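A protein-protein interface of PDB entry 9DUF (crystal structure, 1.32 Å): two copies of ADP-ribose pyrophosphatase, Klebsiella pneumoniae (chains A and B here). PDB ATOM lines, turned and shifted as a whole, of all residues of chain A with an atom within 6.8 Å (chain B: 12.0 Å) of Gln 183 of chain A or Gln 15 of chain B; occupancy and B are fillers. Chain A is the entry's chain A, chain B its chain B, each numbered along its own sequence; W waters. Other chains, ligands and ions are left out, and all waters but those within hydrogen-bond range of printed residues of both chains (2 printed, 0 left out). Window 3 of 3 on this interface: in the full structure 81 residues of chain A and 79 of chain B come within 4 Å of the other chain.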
ATOM      1  N   VAL A  80      -6.508   7.808  -1.033  1.00  0.00           N
ATOM      2  CA  VAL A  80      -7.958   7.761  -1.087  1.00  0.00           C
ATOM      3  C   VAL A  80      -8.406   7.942  -2.528  1.00  0.00           C
ATOM      4  O   VAL A  80      -7.757   8.613  -3.346  1.00  0.00           O
ATOM      5  CB  VAL A  80      -8.649   8.793  -0.175  1.00  0.00           C
ATOM      6  CG1 VAL A  80      -8.262   8.573   1.285  1.00  0.00           C
ATOM      7  CG2 VAL A  80      -8.325  10.208  -0.618  1.00  0.00           C
ATOM      8  N   LEU A 100     -15.869  16.899  -5.547  1.00  0.00           N
ATOM      9  CA  LEU A 100     -15.106  15.700  -5.192  1.00  0.00           C
ATOM     10  C   LEU A 100     -15.743  15.076  -3.948  1.00  0.00           C
ATOM     11  O   LEU A 100     -15.901  15.745  -2.924  1.00  0.00           O
ATOM     12  CB  LEU A 100     -13.662  16.089  -4.892  1.00  0.00           C
ATOM     13  CG  LEU A 100     -12.895  16.724  -6.044  1.00  0.00           C
ATOM     14  CD1 LEU A 100     -11.609  17.343  -5.588  1.00  0.00           C
ATOM     15  CD2 LEU A 100     -12.643  15.687  -7.130  1.00  0.00           C
ATOM     16  N   HIS A 177     -10.661  10.019  -9.143  1.00  0.00           N
ATOM     17  CA  HIS A 177      -9.402  10.669  -8.828  1.00  0.00           C
ATOM     18  C   HIS A 177      -8.748   9.906  -7.693  1.00  0.00           C
ATOM     19  O   HIS A 177      -9.426   9.457  -6.775  1.00  0.00           O
ATOM     20  CB  HIS A 177      -9.606  12.098  -8.342  1.00  0.00           C
ATOM     21  CG  HIS A 177     -10.266  12.996  -9.336  1.00  0.00           C
ATOM     22  ND1 HIS A 177      -9.567  13.931 -10.063  1.00  0.00           N
ATOM     23  CD2 HIS A 177     -11.570  13.149  -9.674  1.00  0.00           C
ATOM     24  CE1 HIS A 177     -10.405  14.593 -10.841  1.00  0.00           C
ATOM     25  NE2 HIS A 177     -11.630  14.145 -10.615  1.00  0.00           N
ATOM     26  N   VAL A 178      -7.433   9.753  -7.755  1.00  0.00           N
ATOM     27  CA  VAL A 178      -6.657   9.168  -6.669  1.00  0.00           C
ATOM     28  C   VAL A 178      -5.706  10.231  -6.148  1.00  0.00           C
ATOM     29  O   VAL A 178      -4.968  10.847  -6.928  1.00  0.00           O
ATOM     30  CB  VAL A 178      -5.879   7.920  -7.123  1.00  0.00           C
ATOM     31  CG1 VAL A 178      -5.011   7.395  -5.969  1.00  0.00           C
ATOM     32  CG2 VAL A 178      -6.839   6.836  -7.611  1.00  0.00           C
ATOM     33  N   VAL A 179      -5.712  10.436  -4.829  1.00  0.00           N
ATOM     34  CA  VAL A 179      -4.797  11.367  -4.187  1.00  0.00           C
ATOM     35  C   VAL A 179      -4.304  10.743  -2.895  1.00  0.00           C
ATOM     36  O   VAL A 179      -4.892   9.799  -2.376  1.00  0.00           O
ATOM     37  CB  VAL A 179      -5.422  12.751  -3.922  1.00  0.00           C
ATOM     38  CG1 VAL A 179      -5.811  13.440  -5.242  1.00  0.00           C
ATOM     39  CG2 VAL A 179      -6.610  12.617  -3.013  1.00  0.00           C
ATOM     40  N   SER A 180      -3.212  11.281  -2.377  1.00  0.00           N
ATOM     41  CA  SER A 180      -2.776  10.888  -1.049  1.00  0.00           C
ATOM     42  C   SER A 180      -3.838  11.280  -0.023  1.00  0.00           C
ATOM     43  O   SER A 180      -4.604  12.232  -0.206  1.00  0.00           O
ATOM     44  CB  SER A 180      -1.462  11.580  -0.720  1.00  0.00           C
ATOM     45  OG  SER A 180      -1.642  12.965  -0.591  1.00  0.00           O
ATOM     46  N   ARG A 181      -3.895  10.531   1.072  1.00  0.00           N
ATOM     47  CA  ARG A 181      -4.714  10.954   2.198  1.00  0.00           C
ATOM     48  C   ARG A 181      -4.386  12.382   2.608  1.00  0.00           C
ATOM     49  O   ARG A 181      -5.293  13.195   2.835  1.00  0.00           O
ATOM     50  CB  ARG A 181      -4.511  10.003   3.373  1.00  0.00           C
ATOM     51  CG  ARG A 181      -5.117  10.534   4.673  1.00  0.00           C
ATOM     52  CD  ARG A 181      -4.683   9.721   5.879  1.00  0.00           C
ATOM     53  NE  ARG A 181      -3.227   9.599   5.964  1.00  0.00           N
ATOM     54  CZ  ARG A 181      -2.405  10.565   6.346  1.00  0.00           C
ATOM     55  NH1 ARG A 181      -2.862  11.740   6.739  1.00  0.00           N
ATOM     56  NH2 ARG A 181      -1.090  10.374   6.248  1.00  0.00           N
ATOM     57  N   GLU A 182      -3.096  12.722   2.677  1.00  0.00           N
ATOM     58  CA  GLU A 182      -2.731  14.048   3.159  1.00  0.00           C
ATOM     59  C   GLU A 182      -3.259  15.122   2.219  1.00  0.00           C
ATOM     60  O   GLU A 182      -3.734  16.168   2.668  1.00  0.00           O
ATOM     61  CB  GLU A 182      -1.220  14.181   3.353  1.00  0.00           C
ATOM     62  CG  GLU A 182      -0.652  13.419   4.557  1.00  0.00           C
ATOM     63  CD  GLU A 182      -0.958  14.041   5.934  1.00  0.00           C
ATOM     64  OE1 GLU A 182      -1.752  15.001   6.038  1.00  0.00           O
ATOM     65  OE2 GLU A 182      -0.384  13.541   6.935  1.00  0.00           O
ATOM     66  N   GLN A 183      -3.198  14.878   0.907  1.00  0.00           N
ATOM     67  CA  GLN A 183      -3.737  15.839  -0.046  1.00  0.00           C
ATOM     68  C   GLN A 183      -5.244  15.969   0.104  1.00  0.00           C
ATOM     69  O   GLN A 183      -5.783  17.080   0.060  1.00  0.00           O
ATOM     70  CB  GLN A 183      -3.373  15.429  -1.472  1.00  0.00           C
ATOM     71  CG  GLN A 183      -3.995  16.345  -2.532  1.00  0.00           C
ATOM     72  CD  GLN A 183      -3.457  17.758  -2.479  1.00  0.00           C
ATOM     73  OE1 GLN A 183      -3.981  18.629  -1.761  1.00  0.00           O
ATOM     74  NE2 GLN A 183      -2.424  18.007  -3.260  1.00  0.00           N
ATOM     75  N   ALA A 184      -5.942  14.850   0.251  1.00  0.00           N
ATOM     76  CA  ALA A 184      -7.388  14.929   0.416  1.00  0.00           C
ATOM     77  C   ALA A 184      -7.750  15.720   1.659  1.00  0.00           C
ATOM     78  O   ALA A 184      -8.660  16.553   1.631  1.00  0.00           O
ATOM     79  CB  ALA A 184      -7.989  13.533   0.480  1.00  0.00           C
ATOM     80  N   TYR A 185      -7.036  15.485   2.759  1.00  0.00           N
ATOM     81  CA  TYR A 185      -7.315  16.229   3.987  1.00  0.00           C
ATOM     82  C   TYR A 185      -6.965  17.711   3.832  1.00  0.00           C
ATOM     83  O   TYR A 185      -7.725  18.576   4.285  1.00  0.00           O
ATOM     84  CB  TYR A 185      -6.585  15.599   5.175  1.00  0.00           C
ATOM     85  CG  TYR A 185      -6.853  16.372   6.427  1.00  0.00           C
ATOM     86  CD1 TYR A 185      -8.112  16.344   6.999  1.00  0.00           C
ATOM     87  CD2 TYR A 185      -5.886  17.181   7.009  1.00  0.00           C
ATOM     88  CE1 TYR A 185      -8.406  17.082   8.130  1.00  0.00           C
ATOM     89  CE2 TYR A 185      -6.164  17.922   8.146  1.00  0.00           C
ATOM     90  CZ  TYR A 185      -7.428  17.870   8.694  1.00  0.00           C
ATOM     91  OH  TYR A 185      -7.725  18.605   9.805  1.00  0.00           O
ATOM     92  N   GLN A 186      -5.833  18.028   3.188  1.00  0.00           N
ATOM     93  CA  GLN A 186      -5.504  19.421   2.892  1.00  0.00           C
ATOM     94  C   GLN A 186      -6.622  20.083   2.090  1.00  0.00           C
ATOM     95  O   GLN A 186      -6.977  21.241   2.333  1.00  0.00           O
ATOM     96  CB  GLN A 186      -4.167  19.504   2.151  1.00  0.00           C
ATOM     97  CG  GLN A 186      -3.730  20.924   1.761  1.00  0.00           C
ATOM     98  CD  GLN A 186      -2.574  20.948   0.746  1.00  0.00           C
ATOM     99  OE1 GLN A 186      -2.704  21.517  -0.353  1.00  0.00           O
ATOM    100  NE2 GLN A 186      -1.442  20.340   1.112  1.00  0.00           N
ATOM    101  N   TRP A 187      -7.226  19.347   1.160  1.00  0.00           N
ATOM    102  CA  TRP A 187      -8.332  19.915   0.392  1.00  0.00           C
ATOM    103  C   TRP A 187      -9.569  20.159   1.249  1.00  0.00           C
ATOM    104  O   TRP A 187     -10.320  21.113   0.995  1.00  0.00           O
ATOM    105  CB  TRP A 187      -8.659  19.032  -0.809  1.00  0.00           C
ATOM    106  CG  TRP A 187      -7.703  19.184  -1.947  1.00  0.00           C
ATOM    107  CD1 TRP A 187      -6.782  20.180  -2.126  1.00  0.00           C
ATOM    108  CD2 TRP A 187      -7.582  18.321  -3.080  1.00  0.00           C
ATOM    109  NE1 TRP A 187      -6.107  19.991  -3.299  1.00  0.00           N
ATOM    110  CE2 TRP A 187      -6.570  18.849  -3.901  1.00  0.00           C
ATOM    111  CE3 TRP A 187      -8.236  17.155  -3.479  1.00  0.00           C
ATOM    112  CZ2 TRP A 187      -6.188  18.242  -5.093  1.00  0.00           C
ATOM    113  CZ3 TRP A 187      -7.867  16.561  -4.659  1.00  0.00           C
ATOM    114  CH2 TRP A 187      -6.853  17.106  -5.458  1.00  0.00           C
ATOM    115  N   VAL A 188      -9.796  19.340   2.273  1.00  0.00           N
ATOM    116  CA  VAL A 188     -10.825  19.682   3.251  1.00  0.00           C
ATOM    117  C   VAL A 188     -10.469  20.984   3.961  1.00  0.00           C
ATOM    118  O   VAL A 188     -11.297  21.888   4.080  1.00  0.00           O
ATOM    119  CB  VAL A 188     -11.044  18.530   4.248  1.00  0.00           C
ATOM    120  CG1 VAL A 188     -11.915  18.990   5.392  1.00  0.00           C
ATOM    121  CG2 VAL A 188     -11.657  17.328   3.546  1.00  0.00           C
ATOM    122  N   GLU A 190      -8.673  23.428   3.016  1.00  0.00           N
ATOM    123  CA  GLU A 190      -8.707  24.542   2.083  1.00  0.00           C
ATOM    124  C   GLU A 190     -10.098  24.827   1.523  1.00  0.00           C
ATOM    125  O   GLU A 190     -10.269  25.832   0.817  1.00  0.00           O
ATOM    126  CB  GLU A 190      -7.763  24.249   0.910  1.00  0.00           C
ATOM    127  CG  GLU A 190      -6.299  24.234   1.291  1.00  0.00           C
ATOM    128  CD  GLU A 190      -5.392  23.721   0.193  1.00  0.00           C
ATOM    129  OE1 GLU A 190      -5.872  23.443  -0.914  1.00  0.00           O
ATOM    130  OE2 GLU A 190      -4.186  23.599   0.449  1.00  0.00           O
ATOM    131  N   LYS A 192     -11.642  22.920  -0.753  1.00  0.00           N
ATOM    132  CA  LYS A 192     -11.824  22.302  -2.064  1.00  0.00           C
ATOM    133  C   LYS A 192     -12.664  21.029  -1.994  1.00  0.00           C
ATOM    134  O   LYS A 192     -13.229  20.612  -3.002  1.00  0.00           O
ATOM    135  CB  LYS A 192     -10.453  22.009  -2.686  1.00  0.00           C
ATOM    136  CG  LYS A 192      -9.668  23.269  -3.086  1.00  0.00           C
ATOM    137  CD  LYS A 192      -8.237  22.935  -3.491  1.00  0.00           C
ATOM    138  CE  LYS A 192      -7.467  24.159  -3.966  1.00  0.00           C
ATOM    139  NZ  LYS A 192      -7.166  25.111  -2.855  1.00  0.00           N
ATOM    140  N   ILE A 193     -12.707  20.367  -0.845  1.00  0.00           N
ATOM    141  CA  ILE A 193     -13.679  19.324  -0.536  1.00  0.00           C
ATOM    142  C   ILE A 193     -14.527  19.883   0.589  1.00  0.00           C
ATOM    143  O   ILE A 193     -14.001  20.200   1.658  1.00  0.00           O
ATOM    144  CB  ILE A 193     -12.993  18.018  -0.115  1.00  0.00           C
ATOM    145  CG1 ILE A 193     -12.201  17.420  -1.289  1.00  0.00           C
ATOM    146  CG2 ILE A 193     -14.018  17.035   0.439  1.00  0.00           C
ATOM    147  CD1 ILE A 193     -11.395  16.203  -0.904  1.00  0.00           C
ATOM    148  N   GLN B  15      -4.699  18.394 -11.231  1.00  0.00           N
ATOM    149  CA  GLN B  15      -5.385  17.880 -10.049  1.00  0.00           C
ATOM    150  C   GLN B  15      -6.606  18.731  -9.722  1.00  0.00           C
ATOM    151  O   GLN B  15      -6.648  19.922 -10.029  1.00  0.00           O
ATOM    152  CB  GLN B  15      -4.438  17.840  -8.849  1.00  0.00           C
ATOM    153  CG  GLN B  15      -4.254  16.446  -8.262  1.00  0.00           C
ATOM    154  CD  GLN B  15      -3.101  16.373  -7.279  1.00  0.00           C
ATOM    155  OE1 GLN B  15      -2.432  17.375  -7.014  1.00  0.00           O
ATOM    156  NE2 GLN B  15      -2.859  15.184  -6.737  1.00  0.00           N
ATOM    157  N   GLY B  16      -7.597  18.108  -9.097  1.00  0.00           N
ATOM    158  CA  GLY B  16      -8.832  18.791  -8.780  1.00  0.00           C
ATOM    159  C   GLY B  16      -9.885  18.567  -9.843  1.00  0.00           C
ATOM    160  O   GLY B  16      -9.723  17.788 -10.790  1.00  0.00           O
ATOM    161  N   ILE B  17     -10.983  19.303  -9.693  1.00  0.00           N
ATOM    162  CA  ILE B  17     -12.154  19.102 -10.538  1.00  0.00           C
ATOM    163  C   ILE B  17     -11.855  19.473 -11.980  1.00  0.00           C
ATOM    164  O   ILE B  17     -10.863  20.149 -12.277  1.00  0.00           O
ATOM    165  CB  ILE B  17     -13.385  19.860 -10.007  1.00  0.00           C
ATOM    166  CG1 ILE B  17     -13.097  21.363  -9.944  1.00  0.00           C
ATOM    167  CG2 ILE B  17     -13.762  19.302  -8.647  1.00  0.00           C
ATOM    168  CD1 ILE B  17     -14.329  22.214  -9.744  1.00  0.00           C
ATOM    169  N   THR B  18     -12.738  19.048 -12.875  1.00  0.00           N
ATOM    170  CA  THR B  18     -12.519  19.051 -14.315  1.00  0.00           C
ATOM    171  C   THR B  18     -13.239  20.200 -15.013  1.00  0.00           C
ATOM    172  O   THR B  18     -12.720  20.771 -15.983  1.00  0.00           O
ATOM    173  CB  THR B  18     -13.034  17.717 -14.881  1.00  0.00           C
ATOM    174  OG1 THR B  18     -12.354  16.608 -14.268  1.00  0.00           O
ATOM    175  CG2 THR B  18     -12.839  17.653 -16.379  1.00  0.00           C
ATOM    176  N   PHE B  19     -14.417  20.566 -14.524  1.00  0.00           N
ATOM    177  CA  PHE B  19     -15.310  21.455 -15.235  1.00  0.00           C
ATOM    178  C   PHE B  19     -15.719  22.575 -14.295  1.00  0.00           C
ATOM    179  O   PHE B  19     -15.671  22.425 -13.063  1.00  0.00           O
ATOM    180  CB  PHE B  19     -16.541  20.689 -15.682  1.00  0.00           C
ATOM    181  CG  PHE B  19     -16.278  19.652 -16.734  1.00  0.00           C
ATOM    182  CD1 PHE B  19     -15.740  20.003 -17.963  1.00  0.00           C
ATOM    183  CD2 PHE B  19     -16.641  18.338 -16.525  1.00  0.00           C
ATOM    184  CE1 PHE B  19     -15.545  19.052 -18.942  1.00  0.00           C
ATOM    185  CE2 PHE B  19     -16.470  17.390 -17.501  1.00  0.00           C
ATOM    186  CZ  PHE B  19     -15.908  17.729 -18.700  1.00  0.00           C
ATOM    187  N   SER B  20     -16.136  23.690 -14.901  1.00  0.00           N
ATOM    188  CA  SER B  20     -16.457  24.947 -14.234  1.00  0.00           C
ATOM    189  C   SER B  20     -17.881  25.358 -14.605  1.00  0.00           C
ATOM    190  O   SER B  20     -18.585  24.650 -15.317  1.00  0.00           O
ATOM    191  CB  SER B  20     -15.475  26.042 -14.668  1.00  0.00           C
ATOM    192  OG  SER B  20     -15.787  26.499 -15.974  1.00  0.00           O
ATOM    193  N   PHE B  49     -17.706  13.847 -19.006  1.00  0.00           N
ATOM    194  CA  PHE B  49     -16.288  13.521 -18.966  1.00  0.00           C
ATOM    195  C   PHE B  49     -15.803  12.913 -20.274  1.00  0.00           C
ATOM    196  O   PHE B  49     -14.633  13.085 -20.615  1.00  0.00           O
ATOM    197  CB  PHE B  49     -15.986  12.589 -17.786  1.00  0.00           C
ATOM    198  CG  PHE B  49     -16.181  13.245 -16.445  1.00  0.00           C
ATOM    199  CD1 PHE B  49     -15.391  14.324 -16.072  1.00  0.00           C
ATOM    200  CD2 PHE B  49     -17.160  12.808 -15.573  1.00  0.00           C
ATOM    201  CE1 PHE B  49     -15.575  14.945 -14.854  1.00  0.00           C
ATOM    202  CE2 PHE B  49     -17.350  13.435 -14.359  1.00  0.00           C
ATOM    203  CZ  PHE B  49     -16.556  14.514 -14.007  1.00  0.00           C
ATOM    204  N   LEU B 136     -15.056  25.498   8.958  1.00  0.00           N
ATOM    205  CA  LEU B 136     -15.266  24.973   7.619  1.00  0.00           C
ATOM    206  C   LEU B 136     -16.653  25.414   7.200  1.00  0.00           C
ATOM    207  O   LEU B 136     -17.523  25.610   8.045  1.00  0.00           O
ATOM    208  CB  LEU B 136     -15.189  23.422   7.593  1.00  0.00           C
ATOM    209  CG  LEU B 136     -13.880  22.739   7.960  1.00  0.00           C
ATOM    210  CD1 LEU B 136     -14.141  21.273   8.030  1.00  0.00           C
ATOM    211  CD2 LEU B 136     -12.810  23.028   6.940  1.00  0.00           C
HETATM  212  O   HOH W   1      -7.247  15.149  -8.832  1.00  0.00           O
HETATM  213  O   HOH W   2      -1.864  13.355  -4.078  1.00  0.00           O
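Water W1 bridges a ring nitrogen (ND1) of His 177 of chain A (2.9 Å) and the backbone NH of Gly 16 of chain B (3.0 Å).
Water W2 bridges the backbone NH of Ser 180 of chain A (3.0 Å) and the side-chain amide nitrogen of Gln 15 of chain B (3.4 Å).
Hydrophobic or aromatic side chains of chain B within 4 Å of the printed part of chain A: Ile 17 and Leu 136.
Printed residues of chain A that touch a printed residue of chain B: Leu 100, His 177, Val 179, Gln 183, Trp 187 and Val 188.
Among the printed residues, 7 pairs touch across the chains.
Among the printed residues, no Asp or Glu carboxylate lies within 4 Å of a Lys or Arg side-chain nitrogen of the other chain.
Gln 183 of chain A touches just one residue of chain B: Gln 15 (3.8 Å).
Val 179 of chain A touches just one residue of chain B: Gln 15.
No residue of chain B comes within 4 Å of Ser 180 of chain A.
No residue of chain B comes within 4 Å of Arg 181 of chain A.
Of the printed residues of chain A, Gly 16 of chain B touches His 177 (3.3 Å) and Trp 187 (3.8 Å).
Of the printed residues of chain B, Val 188 of chain A touches Leu 136.
Lys 192 of chain A touches none of the printed residues of chain B.
Phe 19 of chain B touches none of the printed residues of chain A.
Among the printed residues, merely in contact across the chains: Leu 100 of chain A with Ile 17 of chain B (3.8 Å), His 177 of chain A with Gly 16 of chain B (3.3 Å), Val 179 of chain A with Gln 15 of chain B (3.7 Å), Gln 183 of chain A with Gln 15 of chain B (3.8 Å), Trp 187 of chain A with Gln 15 of chain B (3.9 Å), Trp 187 of chain A with Gly 16 of chain B (3.8 Å) and Val 188 of chain A with Leu 136 of chain B (3.4 Å).
No position is printed for both chains.
The backbone carbonyl oxygen (O) of Val 179 of chain A is in hydrogen-bond range of the backbone NH (N) of Val 80 of chain A (2.9 Å).
The side-chain amide oxygen of Gln 183 of chain A lies close to the side-chain amide oxygen of Gln 186 of chain A (3.5 Å).
The backbone carbonyl oxygen of Trp 187 of chain A lies within hydrogen-bond range of the backbone NH of Lys 192 of chain A, 2.8 Å away.
The side-chain amide oxygen of Gln 183 of chain A sits at hydrogen-bond distance from the indole nitrogen of Trp 187 of chain A, 3.0 Å away.
The backbone carbonyl oxygen of Trp 187 of chain A lies within hydrogen-bond range of the backbone NH of Ile 193 of chain A, at 3.1 Å.
The side-chain hydroxyl (OG) of Ser 180 of chain A lies within hydrogen-bond range of the backbone NH (N) of Gln 183 of chain A (2.9 Å).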
